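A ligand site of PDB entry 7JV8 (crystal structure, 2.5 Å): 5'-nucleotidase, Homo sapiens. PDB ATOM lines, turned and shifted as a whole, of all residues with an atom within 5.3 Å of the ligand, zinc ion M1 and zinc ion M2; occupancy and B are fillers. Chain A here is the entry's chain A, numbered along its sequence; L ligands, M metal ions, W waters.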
ATOM      1  N   ASP A  14     -16.981   3.372   8.320  1.00  0.00           N
ATOM      2  CA  ASP A  14     -17.655   2.148   7.912  1.00  0.00           C
ATOM      3  C   ASP A  14     -17.244   0.934   8.746  1.00  0.00           C
ATOM      4  O   ASP A  14     -16.941  -0.148   8.213  1.00  0.00           O
ATOM      5  CB  ASP A  14     -17.428   1.896   6.416  1.00  0.00           C
ATOM      6  CG  ASP A  14     -17.948   3.036   5.578  1.00  0.00           C
ATOM      7  OD1 ASP A  14     -17.202   4.022   5.392  1.00  0.00           O
ATOM      8  OD2 ASP A  14     -19.084   2.949   5.075  1.00  0.00           O
ATOM      9  N   HIS A  16     -19.131  -0.731  10.796  1.00  0.00           N
ATOM     10  CA  HIS A  16     -20.188  -1.699  10.480  1.00  0.00           C
ATOM     11  C   HIS A  16     -20.276  -2.875  11.457  1.00  0.00           C
ATOM     12  O   HIS A  16     -20.144  -4.053  11.083  1.00  0.00           O
ATOM     13  CB  HIS A  16     -20.071  -2.167   9.012  1.00  0.00           C
ATOM     14  CG  HIS A  16     -20.618  -1.190   8.028  1.00  0.00           C
ATOM     15  ND1 HIS A  16     -21.916  -0.739   8.097  1.00  0.00           N
ATOM     16  CD2 HIS A  16     -20.070  -0.595   6.953  1.00  0.00           C
ATOM     17  CE1 HIS A  16     -22.138   0.098   7.104  1.00  0.00           C
ATOM     18  NE2 HIS A  16     -21.030   0.206   6.388  1.00  0.00           N
ATOM     19  N   ASP A  63     -21.379   5.174   9.445  1.00  0.00           N
ATOM     20  CA  ASP A  63     -21.608   3.730   9.160  1.00  0.00           C
ATOM     21  C   ASP A  63     -21.000   2.783  10.236  1.00  0.00           C
ATOM     22  O   ASP A  63     -20.394   1.740   9.936  1.00  0.00           O
ATOM     23  CB  ASP A  63     -21.176   3.379   7.708  1.00  0.00           C
ATOM     24  CG  ASP A  63     -22.233   3.703   6.627  1.00  0.00           C
ATOM     25  OD1 ASP A  63     -23.271   4.336   6.942  1.00  0.00           O
ATOM     26  OD2 ASP A  63     -21.974   3.371   5.403  1.00  0.00           O
ATOM     27  N   GLN A  66     -24.810  -1.312  11.744  1.00  0.00           N
ATOM     28  CA  GLN A  66     -25.250  -2.360  10.809  1.00  0.00           C
ATOM     29  C   GLN A  66     -24.093  -3.152  10.215  1.00  0.00           C
ATOM     30  O   GLN A  66     -23.150  -2.567   9.702  1.00  0.00           O
ATOM     31  CB  GLN A  66     -26.127  -1.788   9.686  1.00  0.00           C
ATOM     32  CG  GLN A  66     -27.093  -2.739   9.107  1.00  0.00           C
ATOM     33  CD  GLN A  66     -28.401  -2.847   9.854  1.00  0.00           C
ATOM     34  OE1 GLN A  66     -28.640  -3.865  10.480  1.00  0.00           O
ATOM     35  NE2 GLN A  66     -29.268  -1.841   9.723  1.00  0.00           N
ATOM     36  N   ASN A  95     -25.264   7.087   6.501  1.00  0.00           N
ATOM     37  CA  ASN A  95     -26.596   6.681   6.020  1.00  0.00           C
ATOM     38  C   ASN A  95     -27.209   5.550   6.859  1.00  0.00           C
ATOM     39  O   ASN A  95     -28.411   5.607   7.182  1.00  0.00           O
ATOM     40  CB  ASN A  95     -26.572   6.326   4.521  1.00  0.00           C
ATOM     41  CG  ASN A  95     -25.587   5.209   4.162  1.00  0.00           C
ATOM     42  OD1 ASN A  95     -24.357   5.408   4.197  1.00  0.00           O
ATOM     43  ND2 ASN A  95     -26.103   4.033   3.808  1.00  0.00           N
ATOM     44  N   HIS A  96     -26.380   4.574   7.259  1.00  0.00           N
ATOM     45  CA  HIS A  96     -26.836   3.444   8.079  1.00  0.00           C
ATOM     46  C   HIS A  96     -27.238   3.768   9.522  1.00  0.00           C
ATOM     47  O   HIS A  96     -27.936   2.972  10.160  1.00  0.00           O
ATOM     48  CB  HIS A  96     -25.832   2.269   8.034  1.00  0.00           C
ATOM     49  CG  HIS A  96     -25.819   1.579   6.717  1.00  0.00           C
ATOM     50  ND1 HIS A  96     -26.752   0.625   6.361  1.00  0.00           N
ATOM     51  CD2 HIS A  96     -25.030   1.739   5.639  1.00  0.00           C
ATOM     52  CE1 HIS A  96     -26.520   0.232   5.124  1.00  0.00           C
ATOM     53  NE2 HIS A  96     -25.476   0.878   4.668  1.00  0.00           N
ATOM     54  N   ASP A  99     -31.094   3.594   9.791  1.00  0.00           N
ATOM     55  CA  ASP A  99     -31.731   2.338   9.381  1.00  0.00           C
ATOM     56  C   ASP A  99     -32.926   1.889  10.212  1.00  0.00           C
ATOM     57  O   ASP A  99     -33.866   1.333   9.650  1.00  0.00           O
ATOM     58  CB  ASP A  99     -30.693   1.189   9.342  1.00  0.00           C
ATOM     59  CG  ASP A  99     -29.777   1.265   8.117  1.00  0.00           C
ATOM     60  OD1 ASP A  99     -29.925   2.149   7.257  1.00  0.00           O
ATOM     61  OD2 ASP A  99     -28.884   0.409   8.016  1.00  0.00           O
ATOM     62  N   LEU A 162     -31.368   5.124   0.597  1.00  0.00           N
ATOM     63  CA  LEU A 162     -30.664   4.002   1.272  1.00  0.00           C
ATOM     64  C   LEU A 162     -31.164   3.626   2.663  1.00  0.00           C
ATOM     65  O   LEU A 162     -30.759   2.573   3.163  1.00  0.00           O
ATOM     66  CB  LEU A 162     -29.151   4.297   1.358  1.00  0.00           C
ATOM     67  CG  LEU A 162     -28.461   4.822   0.112  1.00  0.00           C
ATOM     68  CD1 LEU A 162     -26.981   5.050   0.393  1.00  0.00           C
ATOM     69  CD2 LEU A 162     -28.637   3.883  -1.060  1.00  0.00           C
ATOM     70  N   SER A 163     -32.008   4.452   3.298  1.00  0.00           N
ATOM     71  CA  SER A 163     -32.316   4.293   4.731  1.00  0.00           C
ATOM     72  C   SER A 163     -33.767   4.678   5.063  1.00  0.00           C
ATOM     73  O   SER A 163     -34.584   4.870   4.139  1.00  0.00           O
ATOM     74  CB  SER A 163     -31.300   5.121   5.534  1.00  0.00           C
ATOM     75  OG  SER A 163     -31.008   4.522   6.778  1.00  0.00           O
ATOM     76  N   ASN A 164     -34.077   4.789   6.353  1.00  0.00           N
ATOM     77  CA  ASN A 164     -35.359   5.316   6.847  1.00  0.00           C
ATOM     78  C   ASN A 164     -35.196   6.584   7.705  1.00  0.00           C
ATOM     79  O   ASN A 164     -35.455   6.546   8.888  1.00  0.00           O
ATOM     80  CB  ASN A 164     -36.085   4.219   7.628  1.00  0.00           C
ATOM     81  CG  ASN A 164     -36.584   3.119   6.728  1.00  0.00           C
ATOM     82  OD1 ASN A 164     -37.361   3.390   5.823  1.00  0.00           O
ATOM     83  ND2 ASN A 164     -36.113   1.897   6.928  1.00  0.00           N
ATOM     84  N   HIS A 198     -19.731  11.579   5.393  1.00  0.00           N
ATOM     85  CA  HIS A 198     -20.149  10.298   4.845  1.00  0.00           C
ATOM     86  C   HIS A 198     -20.947  10.421   3.559  1.00  0.00           C
ATOM     87  O   HIS A 198     -22.174  10.268   3.532  1.00  0.00           O
ATOM     88  CB  HIS A 198     -20.950   9.532   5.906  1.00  0.00           C
ATOM     89  CG  HIS A 198     -21.073   8.079   5.615  1.00  0.00           C
ATOM     90  ND1 HIS A 198     -20.102   7.175   5.961  1.00  0.00           N
ATOM     91  CD2 HIS A 198     -22.006   7.384   4.914  1.00  0.00           C
ATOM     92  CE1 HIS A 198     -20.446   5.979   5.530  1.00  0.00           C
ATOM     93  NE2 HIS A 198     -21.607   6.077   4.899  1.00  0.00           N
ATOM     94  N   HIS A 221     -18.076   5.864   3.381  1.00  0.00           N
ATOM     95  CA  HIS A 221     -19.168   5.429   2.450  1.00  0.00           C
ATOM     96  C   HIS A 221     -18.685   4.650   1.213  1.00  0.00           C
ATOM     97  O   HIS A 221     -19.242   3.614   0.908  1.00  0.00           O
ATOM     98  CB  HIS A 221     -20.048   6.612   2.050  1.00  0.00           C
ATOM     99  CG  HIS A 221     -21.348   6.257   1.397  1.00  0.00           C
ATOM    100  ND1 HIS A 221     -22.434   5.712   2.069  1.00  0.00           N
ATOM    101  CD2 HIS A 221     -21.769   6.487   0.135  1.00  0.00           C
ATOM    102  CE1 HIS A 221     -23.434   5.593   1.218  1.00  0.00           C
ATOM    103  NE2 HIS A 221     -23.054   6.035   0.044  1.00  0.00           N
ATOM    104  N   SER A 222     -17.663   5.138   0.518  1.00  0.00           N
ATOM    105  CA  SER A 222     -17.073   4.432  -0.633  1.00  0.00           C
ATOM    106  C   SER A 222     -16.028   3.358  -0.275  1.00  0.00           C
ATOM    107  O   SER A 222     -15.491   2.717  -1.178  1.00  0.00           O
ATOM    108  CB  SER A 222     -16.521   5.440  -1.625  1.00  0.00           C
ATOM    109  OG  SER A 222     -15.627   6.350  -0.987  1.00  0.00           O
ATOM    110  N   ASN A 223     -15.710   3.182   1.017  1.00  0.00           N
ATOM    111  CA  ASN A 223     -14.800   2.123   1.513  1.00  0.00           C
ATOM    112  C   ASN A 223     -13.416   2.219   0.872  1.00  0.00           C
ATOM    113  O   ASN A 223     -12.784   1.210   0.521  1.00  0.00           O
ATOM    114  CB  ASN A 223     -15.410   0.706   1.314  1.00  0.00           C
ATOM    115  CG  ASN A 223     -16.638   0.400   2.188  1.00  0.00           C
ATOM    116  OD1 ASN A 223     -17.088  -0.743   2.151  1.00  0.00           O
ATOM    117  ND2 ASN A 223     -17.180   1.363   2.933  1.00  0.00           N
ATOM    118  N   ARG A 332     -20.843  -5.856  -6.949  1.00  0.00           N
ATOM    119  CA  ARG A 332     -21.283  -4.544  -7.487  1.00  0.00           C
ATOM    120  C   ARG A 332     -20.820  -4.268  -8.921  1.00  0.00           C
ATOM    121  O   ARG A 332     -21.291  -3.297  -9.510  1.00  0.00           O
ATOM    122  CB  ARG A 332     -20.805  -3.407  -6.578  1.00  0.00           C
ATOM    123  CG  ARG A 332     -21.180  -3.581  -5.120  1.00  0.00           C
ATOM    124  CD  ARG A 332     -20.906  -2.326  -4.313  1.00  0.00           C
ATOM    125  NE  ARG A 332     -21.419  -2.480  -2.952  1.00  0.00           N
ATOM    126  CZ  ARG A 332     -21.893  -1.514  -2.152  1.00  0.00           C
ATOM    127  NH1 ARG A 332     -21.933  -0.230  -2.534  1.00  0.00           N
ATOM    128  NH2 ARG A 332     -22.325  -1.834  -0.935  1.00  0.00           N
ATOM    129  N   ASN A 368     -30.053  -6.548  -5.123  1.00  0.00           N
ATOM    130  CA  ASN A 368     -29.062  -5.470  -5.158  1.00  0.00           C
ATOM    131  C   ASN A 368     -27.739  -5.960  -4.575  1.00  0.00           C
ATOM    132  O   ASN A 368     -27.702  -6.500  -3.457  1.00  0.00           O
ATOM    133  CB  ASN A 368     -29.555  -4.191  -4.452  1.00  0.00           C
ATOM    134  CG  ASN A 368     -29.936  -4.398  -2.983  1.00  0.00           C
ATOM    135  OD1 ASN A 368     -30.843  -5.175  -2.683  1.00  0.00           O
ATOM    136  ND2 ASN A 368     -29.256  -3.717  -2.070  1.00  0.00           N
ATOM    137  N   GLY A 369     -26.677  -5.839  -5.376  1.00  0.00           N
ATOM    138  CA  GLY A 369     -25.331  -6.300  -5.036  1.00  0.00           C
ATOM    139  C   GLY A 369     -24.736  -5.698  -3.764  1.00  0.00           C
ATOM    140  O   GLY A 369     -24.023  -6.375  -3.033  1.00  0.00           O
ATOM    141  N   GLY A 370     -25.067  -4.436  -3.517  1.00  0.00           N
ATOM    142  CA  GLY A 370     -24.717  -3.748  -2.295  1.00  0.00           C
ATOM    143  C   GLY A 370     -25.344  -4.284  -1.023  1.00  0.00           C
ATOM    144  O   GLY A 370     -24.833  -4.004   0.058  1.00  0.00           O
ATOM    145  N   GLY A 371     -26.446  -5.032  -1.141  1.00  0.00           N
ATOM    146  CA  GLY A 371     -27.024  -5.809  -0.038  1.00  0.00           C
ATOM    147  C   GLY A 371     -26.273  -7.066   0.397  1.00  0.00           C
ATOM    148  O   GLY A 371     -26.613  -7.657   1.418  1.00  0.00           O
ATOM    149  N   ARG A 373     -23.074  -8.224   1.943  1.00  0.00           N
ATOM    150  CA  ARG A 373     -22.209  -7.452   2.847  1.00  0.00           C
ATOM    151  C   ARG A 373     -20.951  -8.130   3.359  1.00  0.00           C
ATOM    152  O   ARG A 373     -20.139  -7.489   4.034  1.00  0.00           O
ATOM    153  CB  ARG A 373     -23.052  -6.995   4.031  1.00  0.00           C
ATOM    154  CG  ARG A 373     -24.303  -6.211   3.662  1.00  0.00           C
ATOM    155  CD  ARG A 373     -24.030  -4.956   2.872  1.00  0.00           C
ATOM    156  NE  ARG A 373     -23.285  -3.971   3.659  1.00  0.00           N
ATOM    157  CZ  ARG A 373     -23.134  -2.688   3.349  1.00  0.00           C
ATOM    158  NH1 ARG A 373     -23.672  -2.155   2.234  1.00  0.00           N
ATOM    159  NH2 ARG A 373     -22.437  -1.907   4.180  1.00  0.00           N
ATOM    160  N   PHE A 395     -29.239  -6.818   7.552  1.00  0.00           N
ATOM    161  CA  PHE A 395     -30.266  -5.737   7.657  1.00  0.00           C
ATOM    162  C   PHE A 395     -31.603  -6.131   8.299  1.00  0.00           C
ATOM    163  O   PHE A 395     -32.436  -5.254   8.519  1.00  0.00           O
ATOM    164  CB  PHE A 395     -30.507  -5.105   6.274  1.00  0.00           C
ATOM    165  CG  PHE A 395     -29.260  -4.555   5.642  1.00  0.00           C
ATOM    166  CD1 PHE A 395     -28.559  -3.528   6.242  1.00  0.00           C
ATOM    167  CD2 PHE A 395     -28.752  -5.091   4.451  1.00  0.00           C
ATOM    168  CE1 PHE A 395     -27.371  -3.038   5.691  1.00  0.00           C
ATOM    169  CE2 PHE A 395     -27.577  -4.589   3.872  1.00  0.00           C
ATOM    170  CZ  PHE A 395     -26.895  -3.556   4.501  1.00  0.00           C
ATOM    171  N   SER A 423     -18.868   1.624  -7.827  1.00  0.00           N
ATOM    172  CA  SER A 423     -19.041   0.665  -6.704  1.00  0.00           C
ATOM    173  C   SER A 423     -20.270   0.939  -5.825  1.00  0.00           C
ATOM    174  O   SER A 423     -20.221   0.805  -4.584  1.00  0.00           O
ATOM    175  CB  SER A 423     -17.762   0.591  -5.845  1.00  0.00           C
ATOM    176  OG  SER A 423     -17.804  -0.541  -4.989  1.00  0.00           O
ATOM    177  N   THR A 424     -21.362   1.308  -6.475  1.00  0.00           N
ATOM    178  CA  THR A 424     -22.646   1.578  -5.820  1.00  0.00           C
ATOM    179  C   THR A 424     -23.484   0.307  -5.836  1.00  0.00           C
ATOM    180  O   THR A 424     -23.304  -0.567  -6.677  1.00  0.00           O
ATOM    181  CB  THR A 424     -23.396   2.724  -6.510  1.00  0.00           C
ATOM    182  OG1 THR A 424     -23.513   2.437  -7.919  1.00  0.00           O
ATOM    183  CG2 THR A 424     -22.658   4.026  -6.304  1.00  0.00           C
ATOM    184  N   GLY A 425     -24.408   0.222  -4.877  1.00  0.00           N
ATOM    185  CA  GLY A 425     -25.095  -1.027  -4.573  1.00  0.00           C
ATOM    186  C   GLY A 425     -26.199  -1.480  -5.511  1.00  0.00           C
ATOM    187  O   GLY A 425     -26.578  -2.650  -5.453  1.00  0.00           O
ATOM    188  N   GLU A 426     -26.734  -0.582  -6.348  1.00  0.00           N
ATOM    189  CA  GLU A 426     -27.845  -0.905  -7.268  1.00  0.00           C
ATOM    190  C   GLU A 426     -27.604  -1.982  -8.347  1.00  0.00           C
ATOM    191  O   GLU A 426     -28.566  -2.462  -8.933  1.00  0.00           O
ATOM    192  CB  GLU A 426     -28.419   0.358  -7.948  1.00  0.00           C
ATOM    193  CG  GLU A 426     -27.528   1.091  -8.961  1.00  0.00           C
ATOM    194  CD  GLU A 426     -26.568   2.113  -8.355  1.00  0.00           C
ATOM    195  OE1 GLU A 426     -26.495   2.233  -7.114  1.00  0.00           O
ATOM    196  OE2 GLU A 426     -25.887   2.822  -9.124  1.00  0.00           O
ATOM    197  N   PRO A 476     -35.616  -8.182  -2.530  1.00  0.00           N
ATOM    198  CA  PRO A 476     -35.664  -7.670  -1.173  1.00  0.00           C
ATOM    199  C   PRO A 476     -36.741  -6.603  -0.986  1.00  0.00           C
ATOM    200  O   PRO A 476     -36.996  -5.831  -1.933  1.00  0.00           O
ATOM    201  CB  PRO A 476     -34.256  -7.074  -0.958  1.00  0.00           C
ATOM    202  CG  PRO A 476     -33.411  -7.648  -2.044  1.00  0.00           C
ATOM    203  CD  PRO A 476     -34.359  -7.791  -3.192  1.00  0.00           C
ATOM    204  N   PHE A 478     -36.430  -3.899   0.572  1.00  0.00           N
ATOM    205  CA  PHE A 478     -35.653  -2.701   0.256  1.00  0.00           C
ATOM    206  C   PHE A 478     -35.901  -2.197  -1.161  1.00  0.00           C
ATOM    207  O   PHE A 478     -36.184  -1.010  -1.359  1.00  0.00           O
ATOM    208  CB  PHE A 478     -34.148  -2.989   0.459  1.00  0.00           C
ATOM    209  CG  PHE A 478     -33.253  -1.794   0.191  1.00  0.00           C
ATOM    210  CD1 PHE A 478     -33.348  -0.636   0.974  1.00  0.00           C
ATOM    211  CD2 PHE A 478     -32.308  -1.832  -0.832  1.00  0.00           C
ATOM    212  CE1 PHE A 478     -32.523   0.461   0.738  1.00  0.00           C
ATOM    213  CE2 PHE A 478     -31.485  -0.744  -1.074  1.00  0.00           C
ATOM    214  CZ  PHE A 478     -31.575   0.401  -0.292  1.00  0.00           C
ATOM    215  N   ASP A 484     -32.359   2.011  -3.139  1.00  0.00           N
ATOM    216  CA  ASP A 484     -31.269   2.099  -4.122  1.00  0.00           C
ATOM    217  C   ASP A 484     -31.614   2.898  -5.389  1.00  0.00           C
ATOM    218  O   ASP A 484     -30.987   2.690  -6.442  1.00  0.00           O
ATOM    219  CB  ASP A 484     -30.724   0.665  -4.450  1.00  0.00           C
ATOM    220  CG  ASP A 484     -29.374   0.359  -3.813  1.00  0.00           C
ATOM    221  OD1 ASP A 484     -28.684   1.254  -3.289  1.00  0.00           O
ATOM    222  OD2 ASP A 484     -28.991  -0.810  -3.850  1.00  0.00           O
HETATM  223  C1  LIG L   1     -22.278   1.408   0.896  1.00  0.00           C
HETATM  224  C2  LIG L   1     -20.918   0.682   0.911  1.00  0.00           C
HETATM  225  C3  LIG L   1     -22.187   2.675   0.033  1.00  0.00           C
HETATM  226  O1  LIG L   1     -21.772   2.385  -1.293  1.00  0.00           O
HETATM  227  C4  LIG L   1     -24.502   0.934  -0.072  1.00  0.00           C
HETATM  228  C5  LIG L   1     -27.121  -1.539   0.401  1.00  0.00           C
HETATM  229  C6  LIG L   1     -29.941  -1.592   2.659  1.00  0.00           C
HETATM  230  C7  LIG L   1     -32.227  -0.569   4.420  1.00  0.00           C
HETATM  231  C8  LIG L   1     -32.295  -1.077   6.764  1.00  0.00           C
HETATM  232  C9  LIG L   1     -30.492  -4.038   1.575  1.00  0.00           C
HETATM  233  C10 LIG L   1     -29.130  -2.174   1.644  1.00  0.00           C
HETATM  234  C11 LIG L   1     -27.609  -0.830  -0.887  1.00  0.00           C
HETATM  235  C12 LIG L   1     -26.711   0.397  -0.917  1.00  0.00           C
HETATM  236  O2  LIG L   1     -21.553   2.726   3.076  1.00  0.00           O
HETATM  237  P1  LIG L   1     -22.702   1.910   2.598  1.00  0.00           P
HETATM  238  O3  LIG L   1     -24.027   2.803   2.607  1.00  0.00           O
HETATM  239  O4  LIG L   1     -22.956   0.646   3.525  1.00  0.00           O
HETATM  240  O5  LIG L   1     -20.927  -0.413   1.825  1.00  0.00           O
HETATM  241  C13 LIG L   1     -21.662   3.559  -2.109  1.00  0.00           C
HETATM  242  O6  LIG L   1     -23.257   0.466   0.457  1.00  0.00           O
HETATM  243  C14 LIG L   1     -25.430  -0.215  -0.379  1.00  0.00           C
HETATM  244  O7  LIG L   1     -25.867  -0.929   0.796  1.00  0.00           O
HETATM  245  N1  LIG L   1     -28.128  -1.303   1.408  1.00  0.00           N
HETATM  246  N2  LIG L   1     -28.267  -0.191   2.213  1.00  0.00           N
HETATM  247  C15 LIG L   1     -29.319  -0.349   2.959  1.00  0.00           C
HETATM  248  C16 LIG L   1     -31.069  -2.352   3.090  1.00  0.00           C
HETATM  249  N3  LIG L   1     -32.005  -1.971   4.037  1.00  0.00           N
HETATM  250  C17 LIG L   1     -33.659  -0.231   4.887  1.00  0.00           C
HETATM  251  C18 LIG L   1     -33.747  -0.729   6.354  1.00  0.00           C
HETATM  252  C19 LIG L   1     -31.462  -0.330   5.702  1.00  0.00           C
HETATM  253  N4  LIG L   1     -31.295  -3.538   2.510  1.00  0.00           N
HETATM  254 CL1  LIG L   1     -30.864  -5.578   0.880  1.00  0.00          CL
HETATM  255  N5  LIG L   1     -29.444  -3.378   1.130  1.00  0.00           N
HETATM  256  O8  LIG L   1     -27.370  -1.657  -2.036  1.00  0.00           O
HETATM  257  O9  LIG L   1     -26.507   0.895  -2.238  1.00  0.00           O
HETATM  258 ZN    ZN M   1     -20.720   1.806   4.919  1.00  0.00          ZN
HETATM  259 ZN    ZN M   2     -22.561   4.571   3.836  1.00  0.00          ZN
HETATM  260  O   HOH W   1     -34.634  -3.303   4.467  1.00  0.00           O
HETATM  261  O   HOH W   2     -19.344  -2.066  -0.100  1.00  0.00           O
HETATM  262  O   HOH W   3     -28.988  -7.706   2.576  1.00  0.00           O
HETATM  263  O   HOH W   4     -18.953   2.043  -2.210  1.00  0.00           O
HETATM  264  O   HOH W   5     -19.337   0.425   4.062  1.00  0.00           O
HETATM  265  O   HOH W   6     -31.186  -8.394   0.851  1.00  0.00           O
HETATM  266  O   HOH W   7     -25.397   2.952  -3.387  1.00  0.00           O
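N of Gly 425 sits close to O9 of the ligand (3.4 Å). The side-chain carboxylate (OD1) of Asp 484 is in hydrogen-bond range of an oxygen (O9) of the ligand (2.4 Å). An oxygen (O4) of the ligand is in salt-bridge range of the guanidinium group (NH2) of Arg 373. NH2 of Arg 332 sits at hydrogen-bond distance from O6 of the ligand (2.8 Å). A ring nitrogen (NE2) of His 96 sits at hydrogen-bond distance from an oxygen (O4) of the ligand, at 2.8 Å. The side-chain amide nitrogen (ND2) of Asn 368 is in hydrogen-bond range of an oxygen (O8) of the ligand (2.8 Å).
A ring nitrogen (ND1) of His 96 lies within hydrogen-bond range of the side-chain carboxylate (OD2) of Asp 99. OG of Ser 163 lies within hydrogen-bond range of O of Asn 95 (2.8 Å). The backbone NH of Gly 371 sits close to the side-chain amide nitrogen of Asn 368 (3.2 Å). N of Gly 370 lies within hydrogen-bond range of O of Gly 425 (3.0 Å). A ring nitrogen (ND1) of His 16 sits at hydrogen-bond distance from the backbone carbonyl oxygen (O) of Gln 66 (2.7 Å). OD1 of Asp 63 sits at hydrogen-bond distance from N of His 96, at 3.1 Å. NE2 of His 96 sits close to ND2 of Asn 95, 3.3 Å away. O of Ser 423 sits at hydrogen-bond distance from NH1 of Arg 332 (2.9 Å).
O of Gly 370 sits close to O7 of the ligand (3.3 Å). Merely in contact with the ligand: Asp 99, Leu 162, Asn 164, Asn 223, Gly 371, Phe 395, Ser 423 and Phe 478. Hydrophobic or aromatic side chains within 4 Å of the ligand: His 16, His 96, Leu 162, His 221, Phe 395 and Phe 478.
The nearest printed residue that does not touch zinc ion M1 is Asn 223 (4.1 Å).
The nearest printed residue that does not touch zinc ion M2 is Asp 14 (4.03 Å).
Zinc ion M1 is bound by OD2 of Asp 14 (2.0 Å), OD2 of Asp 63 (2.1 Å), water W5 (2.1 Å), NE2 of His 16 (2.2 Å) and O2 of the ligand (2.2 Å).
Zinc ion M2 is bound by OD1 of Asn 95, OD2 of Asp 63, NE2 of His 198, ND1 of His 221 and O2 of the ligand. Zinc ion M2 has five donor atoms within binding distance. Slightly farther from zinc ion M2 lies O3 of the ligand (2.6 Å).
Water W5 lies within hydrogen-bond range of the side-chain amide nitrogen (ND2) of Asn 223 (2.6 Å) and an oxygen (O5) of the ligand (2.9 Å). Water W7 lies within hydrogen-bond range of an oxygen (O9) of the ligand (2.6 Å) and the backbone NH (N) of Gly 425 (3.3 Å). Water W4 lies within hydrogen-bond range of O of Ser 423 and O1 of the ligand. Water W2 lies within hydrogen-bond range of O5 of the ligand, NH2 of Arg 332 and OD1 of Asn 223.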
